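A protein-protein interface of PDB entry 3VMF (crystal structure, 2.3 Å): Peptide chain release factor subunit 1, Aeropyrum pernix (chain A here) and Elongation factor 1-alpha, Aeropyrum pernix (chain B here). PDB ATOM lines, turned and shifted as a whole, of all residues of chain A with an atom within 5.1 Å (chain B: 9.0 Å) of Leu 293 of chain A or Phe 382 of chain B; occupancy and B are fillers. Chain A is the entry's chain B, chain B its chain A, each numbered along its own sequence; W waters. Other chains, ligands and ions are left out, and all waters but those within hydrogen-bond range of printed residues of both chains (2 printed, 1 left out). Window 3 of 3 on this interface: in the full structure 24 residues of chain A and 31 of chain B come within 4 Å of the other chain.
Among the printed residues, pairs that only touch across the chains: Phe 359 of chain A with Gln 381 of chain B (3.3 Å), Lys 290 of chain A with Ser 340 of chain B (3.3 Å), Trp 354 of chain A with Thr 343 of chain B (3.5 Å), Ala 294 of chain A with Ser 340 of chain B (3.5 Å), Leu 293 of chain A with Phe 382 of chain B (3.6 Å), Trp 354 of chain A with Val 344 of chain B (3.6 Å), Ala 294 of chain A with Lys 384 of chain B (3.7 Å), Leu 293 of chain A with Gln 381 of chain B (3.7 Å), Leu 291 of chain A with Ser 340 of chain B (3.7 Å) and Ala 294 of chain A with Phe 382 of chain B (3.96 Å).
Water W1 lies within hydrogen-bond range of a ring nitrogen (NE2) of His 338 of chain B (2.7 Å) and the side-chain amino group of Lys 290 of chain A (3.4 Å).
Water W2 lies within hydrogen-bond range of the backbone NH (N) of Trp 354 of chain A (2.8 Å) and the backbone carbonyl oxygen (O) of Val 344 of chain B (3.1 Å).
The backbone NH of Ala 341 of chain B sits at hydrogen-bond distance from a ring nitrogen (ND1) of His 338 of chain B.
The backbone NH (N) of Lys 384 of chain B is in hydrogen-bond range of the side-chain carboxylate (OD2) of Asp 387 of chain B (2.8 Å).
ND1 of His 338 of chain B is in hydrogen-bond range of N of Ser 340 of chain B.
The backbone carbonyl oxygen (O) of Ala 341 of chain B is in hydrogen-bond range of the side-chain amino group (NZ) of Lys 290 of chain A (3.0 Å).
The backbone carbonyl oxygen of Gln 381 of chain B sits at hydrogen-bond distance from the indole nitrogen of Trp 354 of chain A.
Of the 11 printed residues of chain A, 6 touch a printed residue of chain B.
Printed residues of chain A that touch a printed residue of chain B: Lys 290, Leu 291, Leu 293, Ala 294, Trp 354 and Phe 359.
Hydrophobic or aromatic side chains of chain A within 4 Å of the printed part of chain B: Leu 293, Ala 294, Trp 354 and Phe 359.
Hydrophobic or aromatic side chains of chain B within 4 Å of the printed part of chain A: Ala 341 and Phe 382.
Among the printed residues, 12 pairs touch across the chains.
Among the printed residues, no Asp or Glu carboxylate lies within 4 Å of a Lys or Arg side-chain nitrogen of the other chain.
Of the printed residues of chain A, Ala 341 of chain B touches Lys 290 (3.0 Å).
Of the printed residues of chain A, Thr 343 of chain B touches Trp 354 (3.5 Å).
Lys 367 of chain B touches none of the printed residues of chain A.
Pro 380 of chain B touches none of the printed residues of chain A.
Phe 382 of chain B touches just these residues of chain A: Leu 293 and Ala 294.
Printed residues of chain A within 4 Å of Lys 384 of chain B: Ala 294 (3.7 Å).
The nearest printed residue of chain B that does not touch Leu 291 of chain A is Ala 341 of chain B (4.9 Å).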
ATOM      1  N   PHE A 289      13.415 -38.142  29.017  1.00  0.00           N
ATOM      2  CA  PHE A 289      13.219 -37.155  27.965  1.00  0.00           C
ATOM      3  C   PHE A 289      12.408 -35.953  28.485  1.00  0.00           C
ATOM      4  O   PHE A 289      12.746 -34.791  28.217  1.00  0.00           O
ATOM      5  CB  PHE A 289      12.519 -37.822  26.780  1.00  0.00           C
ATOM      6  CG  PHE A 289      12.301 -36.925  25.601  1.00  0.00           C
ATOM      7  CD1 PHE A 289      13.353 -36.585  24.767  1.00  0.00           C
ATOM      8  CD2 PHE A 289      11.031 -36.458  25.299  1.00  0.00           C
ATOM      9  CE1 PHE A 289      13.156 -35.761  23.664  1.00  0.00           C
ATOM     10  CE2 PHE A 289      10.819 -35.640  24.203  1.00  0.00           C
ATOM     11  CZ  PHE A 289      11.891 -35.291  23.374  1.00  0.00           C
ATOM     12  N   LYS A 290      11.351 -36.247  29.234  1.00  0.00           N
ATOM     13  CA  LYS A 290      10.472 -35.209  29.759  1.00  0.00           C
ATOM     14  C   LYS A 290      11.117 -34.455  30.910  1.00  0.00           C
ATOM     15  O   LYS A 290      10.950 -33.243  31.016  1.00  0.00           O
ATOM     16  CB  LYS A 290       9.120 -35.787  30.178  1.00  0.00           C
ATOM     17  CG  LYS A 290       8.302 -36.317  29.013  1.00  0.00           C
ATOM     18  CD  LYS A 290       6.877 -36.665  29.430  1.00  0.00           C
ATOM     19  CE  LYS A 290       6.791 -37.922  30.302  1.00  0.00           C
ATOM     20  NZ  LYS A 290       5.350 -38.243  30.579  1.00  0.00           N
ATOM     21  N   LEU A 291      11.851 -35.170  31.757  1.00  0.00           N
ATOM     22  CA  LEU A 291      12.609 -34.552  32.834  1.00  0.00           C
ATOM     23  C   LEU A 291      13.498 -33.461  32.263  1.00  0.00           C
ATOM     24  O   LEU A 291      13.405 -32.305  32.686  1.00  0.00           O
ATOM     25  CB  LEU A 291      13.491 -35.575  33.540  1.00  0.00           C
ATOM     26  CG  LEU A 291      13.532 -35.608  35.072  1.00  0.00           C
ATOM     27  CD1 LEU A 291      14.949 -35.909  35.551  1.00  0.00           C
ATOM     28  CD2 LEU A 291      13.021 -34.323  35.686  1.00  0.00           C
ATOM     29  N   HIS A 292      14.349 -33.837  31.302  1.00  0.00           N
ATOM     30  CA  HIS A 292      15.256 -32.884  30.642  1.00  0.00           C
ATOM     31  C   HIS A 292      14.511 -31.627  30.190  1.00  0.00           C
ATOM     32  O   HIS A 292      14.948 -30.502  30.462  1.00  0.00           O
ATOM     33  CB  HIS A 292      15.995 -33.532  29.463  1.00  0.00           C
ATOM     34  CG  HIS A 292      17.113 -34.441  29.880  1.00  0.00           C
ATOM     35  ND1 HIS A 292      18.197 -34.005  30.612  1.00  0.00           N
ATOM     36  CD2 HIS A 292      17.309 -35.765  29.679  1.00  0.00           C
ATOM     37  CE1 HIS A 292      19.016 -35.016  30.837  1.00  0.00           C
ATOM     38  NE2 HIS A 292      18.496 -36.098  30.288  1.00  0.00           N
ATOM     39  N   LEU A 293      13.370 -31.830  29.536  1.00  0.00           N
ATOM     40  CA  LEU A 293      12.519 -30.719  29.126  1.00  0.00           C
ATOM     41  C   LEU A 293      12.087 -29.845  30.316  1.00  0.00           C
ATOM     42  O   LEU A 293      12.218 -28.628  30.272  1.00  0.00           O
ATOM     43  CB  LEU A 293      11.291 -31.221  28.361  1.00  0.00           C
ATOM     44  CG  LEU A 293      11.517 -31.814  26.965  1.00  0.00           C
ATOM     45  CD1 LEU A 293      10.181 -32.169  26.308  1.00  0.00           C
ATOM     46  CD2 LEU A 293      12.310 -30.837  26.077  1.00  0.00           C
ATOM     47  N   ALA A 294      11.596 -30.477  31.378  1.00  0.00           N
ATOM     48  CA  ALA A 294      11.033 -29.751  32.514  1.00  0.00           C
ATOM     49  C   ALA A 294      12.097 -29.017  33.314  1.00  0.00           C
ATOM     50  O   ALA A 294      11.838 -27.953  33.848  1.00  0.00           O
ATOM     51  CB  ALA A 294      10.222 -30.698  33.425  1.00  0.00           C
ATOM     52  N   LYS A 295      13.292 -29.596  33.398  1.00  0.00           N
ATOM     53  CA  LYS A 295      14.380 -28.973  34.141  1.00  0.00           C
ATOM     54  C   LYS A 295      15.205 -27.985  33.291  1.00  0.00           C
ATOM     55  O   LYS A 295      16.179 -27.406  33.772  1.00  0.00           O
ATOM     56  CB  LYS A 295      15.290 -30.039  34.735  1.00  0.00           C
ATOM     57  CG  LYS A 295      14.577 -31.025  35.632  1.00  0.00           C
ATOM     58  CD  LYS A 295      14.734 -30.669  37.108  1.00  0.00           C
ATOM     59  CE  LYS A 295      13.611 -29.750  37.603  1.00  0.00           C
ATOM     60  NZ  LYS A 295      12.288 -30.451  37.703  1.00  0.00           N
ATOM     61  N   GLY A 296      14.814 -27.812  32.030  1.00  0.00           N
ATOM     62  CA  GLY A 296      15.490 -26.891  31.133  1.00  0.00           C
ATOM     63  C   GLY A 296      16.986 -27.121  31.058  1.00  0.00           C
ATOM     64  O   GLY A 296      17.782 -26.185  31.167  1.00  0.00           O
ATOM     65  N   ILE A 300      18.745 -32.201  24.905  1.00  0.00           N
ATOM     66  CA  ILE A 300      17.913 -32.906  23.946  1.00  0.00           C
ATOM     67  C   ILE A 300      18.105 -32.361  22.534  1.00  0.00           C
ATOM     68  O   ILE A 300      17.811 -31.199  22.257  1.00  0.00           O
ATOM     69  CB  ILE A 300      16.444 -32.739  24.321  1.00  0.00           C
ATOM     70  CG1 ILE A 300      16.108 -33.657  25.493  1.00  0.00           C
ATOM     71  CG2 ILE A 300      15.528 -32.990  23.116  1.00  0.00           C
ATOM     72  CD1 ILE A 300      14.699 -33.525  25.948  1.00  0.00           C
ATOM     73  N   TRP A 354       2.237 -36.921  20.758  1.00  0.00           N
ATOM     74  CA  TRP A 354       2.873 -35.652  21.110  1.00  0.00           C
ATOM     75  C   TRP A 354       4.310 -35.632  20.646  1.00  0.00           C
ATOM     76  O   TRP A 354       4.832 -34.597  20.243  1.00  0.00           O
ATOM     77  CB  TRP A 354       2.832 -35.443  22.625  1.00  0.00           C
ATOM     78  CG  TRP A 354       3.770 -34.417  23.185  1.00  0.00           C
ATOM     79  CD1 TRP A 354       3.537 -33.066  23.314  1.00  0.00           C
ATOM     80  CD2 TRP A 354       5.071 -34.654  23.751  1.00  0.00           C
ATOM     81  NE1 TRP A 354       4.620 -32.456  23.914  1.00  0.00           N
ATOM     82  CE2 TRP A 354       5.573 -33.403  24.187  1.00  0.00           C
ATOM     83  CE3 TRP A 354       5.862 -35.793  23.919  1.00  0.00           C
ATOM     84  CZ2 TRP A 354       6.828 -33.269  24.785  1.00  0.00           C
ATOM     85  CZ3 TRP A 354       7.122 -35.658  24.505  1.00  0.00           C
ATOM     86  CH2 TRP A 354       7.587 -34.409  24.939  1.00  0.00           C
ATOM     87  N   PHE A 359       7.923 -33.148  17.888  1.00  0.00           N
ATOM     88  CA  PHE A 359       9.345 -33.349  17.575  1.00  0.00           C
ATOM     89  C   PHE A 359       9.615 -34.179  16.306  1.00  0.00           C
ATOM     90  O   PHE A 359      10.748 -34.622  16.068  1.00  0.00           O
ATOM     91  CB  PHE A 359      10.079 -33.980  18.755  1.00  0.00           C
ATOM     92  CG  PHE A 359      10.020 -33.169  20.005  1.00  0.00           C
ATOM     93  CD1 PHE A 359       9.091 -33.462  20.992  1.00  0.00           C
ATOM     94  CD2 PHE A 359      10.895 -32.114  20.204  1.00  0.00           C
ATOM     95  CE1 PHE A 359       9.034 -32.715  22.156  1.00  0.00           C
ATOM     96  CE2 PHE A 359      10.844 -31.366  21.366  1.00  0.00           C
ATOM     97  CZ  PHE A 359       9.910 -31.665  22.342  1.00  0.00           C
ATOM     98  N   VAL B 335      -1.362 -28.998  38.936  1.00  0.00           N
ATOM     99  CA  VAL B 335      -0.521 -30.171  39.072  1.00  0.00           C
ATOM    100  C   VAL B 335       0.206 -30.190  40.402  1.00  0.00           C
ATOM    101  O   VAL B 335       1.146 -29.425  40.625  1.00  0.00           O
ATOM    102  CB  VAL B 335       0.524 -30.274  37.947  1.00  0.00           C
ATOM    103  CG1 VAL B 335       1.334 -31.570  38.108  1.00  0.00           C
ATOM    104  CG2 VAL B 335      -0.144 -30.221  36.601  1.00  0.00           C
ATOM    105  N   HIS B 338       4.520 -34.416  39.951  1.00  0.00           N
ATOM    106  CA  HIS B 338       4.881 -35.222  38.795  1.00  0.00           C
ATOM    107  C   HIS B 338       6.394 -35.340  38.642  1.00  0.00           C
ATOM    108  O   HIS B 338       7.119 -34.354  38.728  1.00  0.00           O
ATOM    109  CB  HIS B 338       4.264 -34.665  37.521  1.00  0.00           C
ATOM    110  CG  HIS B 338       4.238 -35.654  36.402  1.00  0.00           C
ATOM    111  ND1 HIS B 338       5.345 -35.925  35.630  1.00  0.00           N
ATOM    112  CD2 HIS B 338       3.251 -36.460  35.947  1.00  0.00           C
ATOM    113  CE1 HIS B 338       5.036 -36.846  34.734  1.00  0.00           C
ATOM    114  NE2 HIS B 338       3.773 -37.187  34.906  1.00  0.00           N
ATOM    115  N   SER B 340       8.235 -35.964  36.081  1.00  0.00           N
ATOM    116  CA  SER B 340       8.839 -35.441  34.854  1.00  0.00           C
ATOM    117  C   SER B 340       7.994 -34.315  34.254  1.00  0.00           C
ATOM    118  O   SER B 340       8.057 -33.174  34.701  1.00  0.00           O
ATOM    119  CB  SER B 340       9.077 -36.571  33.837  1.00  0.00           C
ATOM    120  OG  SER B 340       7.846 -37.065  33.335  1.00  0.00           O
ATOM    121  N   ALA B 341       7.183 -34.644  33.264  1.00  0.00           N
ATOM    122  CA  ALA B 341       6.262 -33.665  32.713  1.00  0.00           C
ATOM    123  C   ALA B 341       5.019 -34.341  32.188  1.00  0.00           C
ATOM    124  O   ALA B 341       5.019 -35.537  31.921  1.00  0.00           O
ATOM    125  CB  ALA B 341       6.919 -32.884  31.604  1.00  0.00           C
ATOM    126  N   ILE B 342       3.965 -33.555  32.037  1.00  0.00           N
ATOM    127  CA  ILE B 342       2.704 -34.029  31.513  1.00  0.00           C
ATOM    128  C   ILE B 342       2.487 -33.435  30.129  1.00  0.00           C
ATOM    129  O   ILE B 342       2.585 -32.239  29.949  1.00  0.00           O
ATOM    130  CB  ILE B 342       1.568 -33.601  32.439  1.00  0.00           C
ATOM    131  CG1 ILE B 342       1.679 -34.362  33.766  1.00  0.00           C
ATOM    132  CG2 ILE B 342       0.212 -33.806  31.777  1.00  0.00           C
ATOM    133  CD1 ILE B 342       0.838 -33.780  34.878  1.00  0.00           C
ATOM    134  N   THR B 343       2.195 -34.271  29.146  1.00  0.00           N
ATOM    135  CA  THR B 343       1.981 -33.778  27.796  1.00  0.00           C
ATOM    136  C   THR B 343       0.588 -34.140  27.319  1.00  0.00           C
ATOM    137  O   THR B 343      -0.122 -34.877  27.986  1.00  0.00           O
ATOM    138  CB  THR B 343       2.982 -34.404  26.808  1.00  0.00           C
ATOM    139  OG1 THR B 343       2.665 -35.785  26.628  1.00  0.00           O
ATOM    140  CG2 THR B 343       4.401 -34.280  27.321  1.00  0.00           C
ATOM    141  N   VAL B 344       0.195 -33.623  26.158  1.00  0.00           N
ATOM    142  CA  VAL B 344      -0.945 -34.182  25.445  1.00  0.00           C
ATOM    143  C   VAL B 344      -0.753 -35.697  25.362  1.00  0.00           C
ATOM    144  O   VAL B 344       0.342 -36.161  25.064  1.00  0.00           O
ATOM    145  CB  VAL B 344      -1.049 -33.594  24.027  1.00  0.00           C
ATOM    146  CG1 VAL B 344      -1.950 -34.466  23.127  1.00  0.00           C
ATOM    147  CG2 VAL B 344      -1.528 -32.122  24.089  1.00  0.00           C
ATOM    148  N   ILE B 361      -5.528 -36.909  28.086  1.00  0.00           N
ATOM    149  CA  ILE B 361      -5.429 -35.486  27.754  1.00  0.00           C
ATOM    150  C   ILE B 361      -5.240 -35.341  26.248  1.00  0.00           C
ATOM    151  O   ILE B 361      -4.172 -35.646  25.712  1.00  0.00           O
ATOM    152  CB  ILE B 361      -4.256 -34.800  28.469  1.00  0.00           C
ATOM    153  CG1 ILE B 361      -4.478 -34.785  29.975  1.00  0.00           C
ATOM    154  CG2 ILE B 361      -4.122 -33.369  27.986  1.00  0.00           C
ATOM    155  CD1 ILE B 361      -3.357 -34.151  30.761  1.00  0.00           C
ATOM    156  N   ILE B 364      -3.839 -29.447  25.632  1.00  0.00           N
ATOM    157  CA  ILE B 364      -3.595 -28.482  26.691  1.00  0.00           C
ATOM    158  C   ILE B 364      -3.794 -27.069  26.114  1.00  0.00           C
ATOM    159  O   ILE B 364      -2.869 -26.482  25.546  1.00  0.00           O
ATOM    160  CB  ILE B 364      -2.165 -28.639  27.231  1.00  0.00           C
ATOM    161  CG1 ILE B 364      -1.900 -30.095  27.639  1.00  0.00           C
ATOM    162  CG2 ILE B 364      -1.932 -27.706  28.392  1.00  0.00           C
ATOM    163  CD1 ILE B 364      -0.453 -30.401  27.930  1.00  0.00           C
ATOM    164  N   ALA B 366      -4.251 -24.033  27.439  1.00  0.00           N
ATOM    165  CA  ALA B 366      -3.476 -22.930  28.016  1.00  0.00           C
ATOM    166  C   ALA B 366      -2.875 -23.238  29.401  1.00  0.00           C
ATOM    167  O   ALA B 366      -3.517 -23.890  30.231  1.00  0.00           O
ATOM    168  CB  ALA B 366      -4.335 -21.673  28.080  1.00  0.00           C
ATOM    169  N   LYS B 367      -1.640 -22.779  29.630  1.00  0.00           N
ATOM    170  CA  LYS B 367      -1.049 -22.742  30.964  1.00  0.00           C
ATOM    171  C   LYS B 367      -1.533 -21.461  31.640  1.00  0.00           C
ATOM    172  O   LYS B 367      -1.591 -20.395  31.014  1.00  0.00           O
ATOM    173  CB  LYS B 367       0.480 -22.706  30.893  1.00  0.00           C
ATOM    174  CG  LYS B 367       1.169 -23.674  31.841  1.00  0.00           C
ATOM    175  CD  LYS B 367       2.276 -23.051  32.681  1.00  0.00           C
ATOM    176  CE  LYS B 367       3.507 -22.683  31.882  1.00  0.00           C
ATOM    177  NZ  LYS B 367       4.153 -23.872  31.272  1.00  0.00           N
ATOM    178  N   LEU B 368      -1.873 -21.556  32.917  1.00  0.00           N
ATOM    179  CA  LEU B 368      -2.314 -20.390  33.666  1.00  0.00           C
ATOM    180  C   LEU B 368      -1.373 -20.122  34.837  1.00  0.00           C
ATOM    181  O   LEU B 368      -0.727 -21.046  35.354  1.00  0.00           O
ATOM    182  CB  LEU B 368      -3.750 -20.592  34.180  1.00  0.00           C
ATOM    183  CG  LEU B 368      -4.834 -21.043  33.188  1.00  0.00           C
ATOM    184  CD1 LEU B 368      -6.159 -21.332  33.882  1.00  0.00           C
ATOM    185  CD2 LEU B 368      -5.023 -20.015  32.100  1.00  0.00           C
ATOM    186  N   GLU B 377       0.541 -18.892  28.627  1.00  0.00           N
ATOM    187  CA  GLU B 377       0.976 -19.486  27.363  1.00  0.00           C
ATOM    188  C   GLU B 377      -0.081 -20.350  26.693  1.00  0.00           C
ATOM    189  O   GLU B 377      -0.581 -21.296  27.290  1.00  0.00           O
ATOM    190  CB  GLU B 377       2.238 -20.317  27.545  1.00  0.00           C
ATOM    191  CG  GLU B 377       2.586 -21.088  26.305  1.00  0.00           C
ATOM    192  CD  GLU B 377       3.992 -21.629  26.324  1.00  0.00           C
ATOM    193  OE1 GLU B 377       4.602 -21.692  27.414  1.00  0.00           O
ATOM    194  OE2 GLU B 377       4.489 -21.986  25.234  1.00  0.00           O
ATOM    195  N   GLN B 378      -0.409 -20.022  25.446  1.00  0.00           N
ATOM    196  CA  GLN B 378      -1.287 -20.858  24.630  1.00  0.00           C
ATOM    197  C   GLN B 378      -0.565 -22.139  24.273  1.00  0.00           C
ATOM    198  O   GLN B 378       0.645 -22.119  24.062  1.00  0.00           O
ATOM    199  CB  GLN B 378      -1.686 -20.137  23.343  1.00  0.00           C
ATOM    200  CG  GLN B 378      -2.611 -18.958  23.559  1.00  0.00           C
ATOM    201  CD  GLN B 378      -3.940 -19.384  24.134  1.00  0.00           C
ATOM    202  OE1 GLN B 378      -4.137 -19.365  25.346  1.00  0.00           O
ATOM    203  NE2 GLN B 378      -4.864 -19.782  23.263  1.00  0.00           N
ATOM    204  N   ASN B 379      -1.323 -23.237  24.206  1.00  0.00           N
ATOM    205  CA  ASN B 379      -0.816 -24.579  23.923  1.00  0.00           C
ATOM    206  C   ASN B 379       0.616 -24.862  24.365  1.00  0.00           C
ATOM    207  O   ASN B 379       1.504 -25.050  23.532  1.00  0.00           O
ATOM    208  CB  ASN B 379      -1.001 -24.911  22.444  1.00  0.00           C
ATOM    209  CG  ASN B 379      -2.452 -24.847  22.018  1.00  0.00           C
ATOM    210  OD1 ASN B 379      -3.165 -25.853  22.032  1.00  0.00           O
ATOM    211  ND2 ASN B 379      -2.904 -23.655  21.648  1.00  0.00           N
ATOM    212  N   PRO B 380       0.847 -24.888  25.682  1.00  0.00           N
ATOM    213  CA  PRO B 380       2.196 -25.176  26.188  1.00  0.00           C
ATOM    214  C   PRO B 380       2.712 -26.523  25.696  1.00  0.00           C
ATOM    215  O   PRO B 380       1.929 -27.432  25.382  1.00  0.00           O
ATOM    216  CB  PRO B 380       2.017 -25.188  27.710  1.00  0.00           C
ATOM    217  CG  PRO B 380       0.558 -25.311  27.953  1.00  0.00           C
ATOM    218  CD  PRO B 380      -0.144 -24.736  26.762  1.00  0.00           C
ATOM    219  N   GLN B 381       4.028 -26.645  25.615  1.00  0.00           N
ATOM    220  CA  GLN B 381       4.616 -27.852  25.068  1.00  0.00           C
ATOM    221  C   GLN B 381       4.397 -28.967  26.080  1.00  0.00           C
ATOM    222  O   GLN B 381       4.288 -30.135  25.713  1.00  0.00           O
ATOM    223  CB  GLN B 381       6.108 -27.666  24.778  1.00  0.00           C
ATOM    224  CG  GLN B 381       6.771 -28.925  24.231  1.00  0.00           C
ATOM    225  CD  GLN B 381       8.272 -28.782  24.063  1.00  0.00           C
ATOM    226  OE1 GLN B 381       8.769 -28.651  22.943  1.00  0.00           O
ATOM    227  NE2 GLN B 381       9.002 -28.811  25.174  1.00  0.00           N
ATOM    228  N   PHE B 382       4.327 -28.580  27.352  1.00  0.00           N
ATOM    229  CA  PHE B 382       4.009 -29.491  28.439  1.00  0.00           C
ATOM    230  C   PHE B 382       3.560 -28.724  29.694  1.00  0.00           C
ATOM    231  O   PHE B 382       3.590 -27.490  29.731  1.00  0.00           O
ATOM    232  CB  PHE B 382       5.225 -30.354  28.772  1.00  0.00           C
ATOM    233  CG  PHE B 382       6.472 -29.567  29.023  1.00  0.00           C
ATOM    234  CD1 PHE B 382       6.752 -29.070  30.288  1.00  0.00           C
ATOM    235  CD2 PHE B 382       7.362 -29.313  27.996  1.00  0.00           C
ATOM    236  CE1 PHE B 382       7.908 -28.329  30.531  1.00  0.00           C
ATOM    237  CE2 PHE B 382       8.519 -28.578  28.225  1.00  0.00           C
ATOM    238  CZ  PHE B 382       8.790 -28.085  29.500  1.00  0.00           C
ATOM    239  N   LEU B 383       3.149 -29.477  30.712  1.00  0.00           N
ATOM    240  CA  LEU B 383       2.910 -28.952  32.044  1.00  0.00           C
ATOM    241  C   LEU B 383       3.886 -29.629  32.990  1.00  0.00           C
ATOM    242  O   LEU B 383       4.387 -30.723  32.705  1.00  0.00           O
ATOM    243  CB  LEU B 383       1.486 -29.256  32.482  1.00  0.00           C
ATOM    244  CG  LEU B 383       0.406 -28.781  31.528  1.00  0.00           C
ATOM    245  CD1 LEU B 383      -0.957 -29.249  31.972  1.00  0.00           C
ATOM    246  CD2 LEU B 383       0.448 -27.258  31.458  1.00  0.00           C
ATOM    247  N   LYS B 384       4.176 -28.982  34.112  1.00  0.00           N
ATOM    248  CA  LYS B 384       4.934 -29.636  35.172  1.00  0.00           C
ATOM    249  C   LYS B 384       4.376 -29.305  36.550  1.00  0.00           C
ATOM    250  O   LYS B 384       3.439 -28.523  36.670  1.00  0.00           O
ATOM    251  CB  LYS B 384       6.435 -29.349  35.087  1.00  0.00           C
ATOM    252  CG  LYS B 384       6.868 -27.895  35.266  1.00  0.00           C
ATOM    253  CD  LYS B 384       8.404 -27.820  35.243  1.00  0.00           C
ATOM    254  CE  LYS B 384       8.941 -26.493  35.789  1.00  0.00           C
ATOM    255  NZ  LYS B 384       8.765 -25.401  34.798  1.00  0.00           N
ATOM    256  N   ALA B 385       4.933 -29.939  37.573  1.00  0.00           N
ATOM    257  CA  ALA B 385       4.500 -29.714  38.944  1.00  0.00           C
ATOM    258  C   ALA B 385       4.531 -28.228  39.266  1.00  0.00           C
ATOM    259  O   ALA B 385       5.549 -27.555  39.078  1.00  0.00           O
ATOM    260  CB  ALA B 385       5.387 -30.491  39.905  1.00  0.00           C
ATOM    261  N   ASP B 387       2.234 -26.132  37.830  1.00  0.00           N
ATOM    262  CA  ASP B 387       1.465 -25.467  36.788  1.00  0.00           C
ATOM    263  C   ASP B 387      -0.020 -25.618  37.017  1.00  0.00           C
ATOM    264  O   ASP B 387      -0.473 -26.596  37.637  1.00  0.00           O
ATOM    265  CB  ASP B 387       1.781 -26.025  35.394  1.00  0.00           C
ATOM    266  CG  ASP B 387       3.183 -25.707  34.942  1.00  0.00           C
ATOM    267  OD1 ASP B 387       3.841 -24.897  35.619  1.00  0.00           O
ATOM    268  OD2 ASP B 387       3.621 -26.267  33.913  1.00  0.00           O
ATOM    269  N   ALA B 388      -0.762 -24.634  36.511  1.00  0.00           N
ATOM    270  CA  ALA B 388      -2.206 -24.714  36.379  1.00  0.00           C
ATOM    271  C   ALA B 388      -2.538 -24.589  34.895  1.00  0.00           C
ATOM    272  O   ALA B 388      -1.755 -24.016  34.142  1.00  0.00           O
ATOM    273  CB  ALA B 388      -2.878 -23.614  37.173  1.00  0.00           C
ATOM    274  N   ALA B 389      -3.680 -25.122  34.464  1.00  0.00           N
ATOM    275  CA  ALA B 389      -3.963 -25.187  33.040  1.00  0.00           C
ATOM    276  C   ALA B 389      -5.435 -25.394  32.745  1.00  0.00           C
ATOM    277  O   ALA B 389      -6.200 -25.733  33.629  1.00  0.00           O
ATOM    278  CB  ALA B 389      -3.139 -26.291  32.391  1.00  0.00           C
ATOM    279  N   VAL B 391      -7.436 -27.829  30.209  1.00  0.00           N
ATOM    280  CA  VAL B 391      -7.096 -28.985  29.372  1.00  0.00           C
ATOM    281  C   VAL B 391      -8.344 -29.697  28.890  1.00  0.00           C
ATOM    282  O   VAL B 391      -9.418 -29.576  29.492  1.00  0.00           O
ATOM    283  CB  VAL B 391      -6.208 -30.013  30.111  1.00  0.00           C
ATOM    284  CG1 VAL B 391      -4.886 -29.395  30.562  1.00  0.00           C
ATOM    285  CG2 VAL B 391      -6.955 -30.620  31.302  1.00  0.00           C
HETATM  286  O   HOH W   1       3.661 -39.394  33.333  1.00  0.00           O
HETATM  287  O   HOH W   2       0.834 -38.219  22.835  1.00  0.00           O
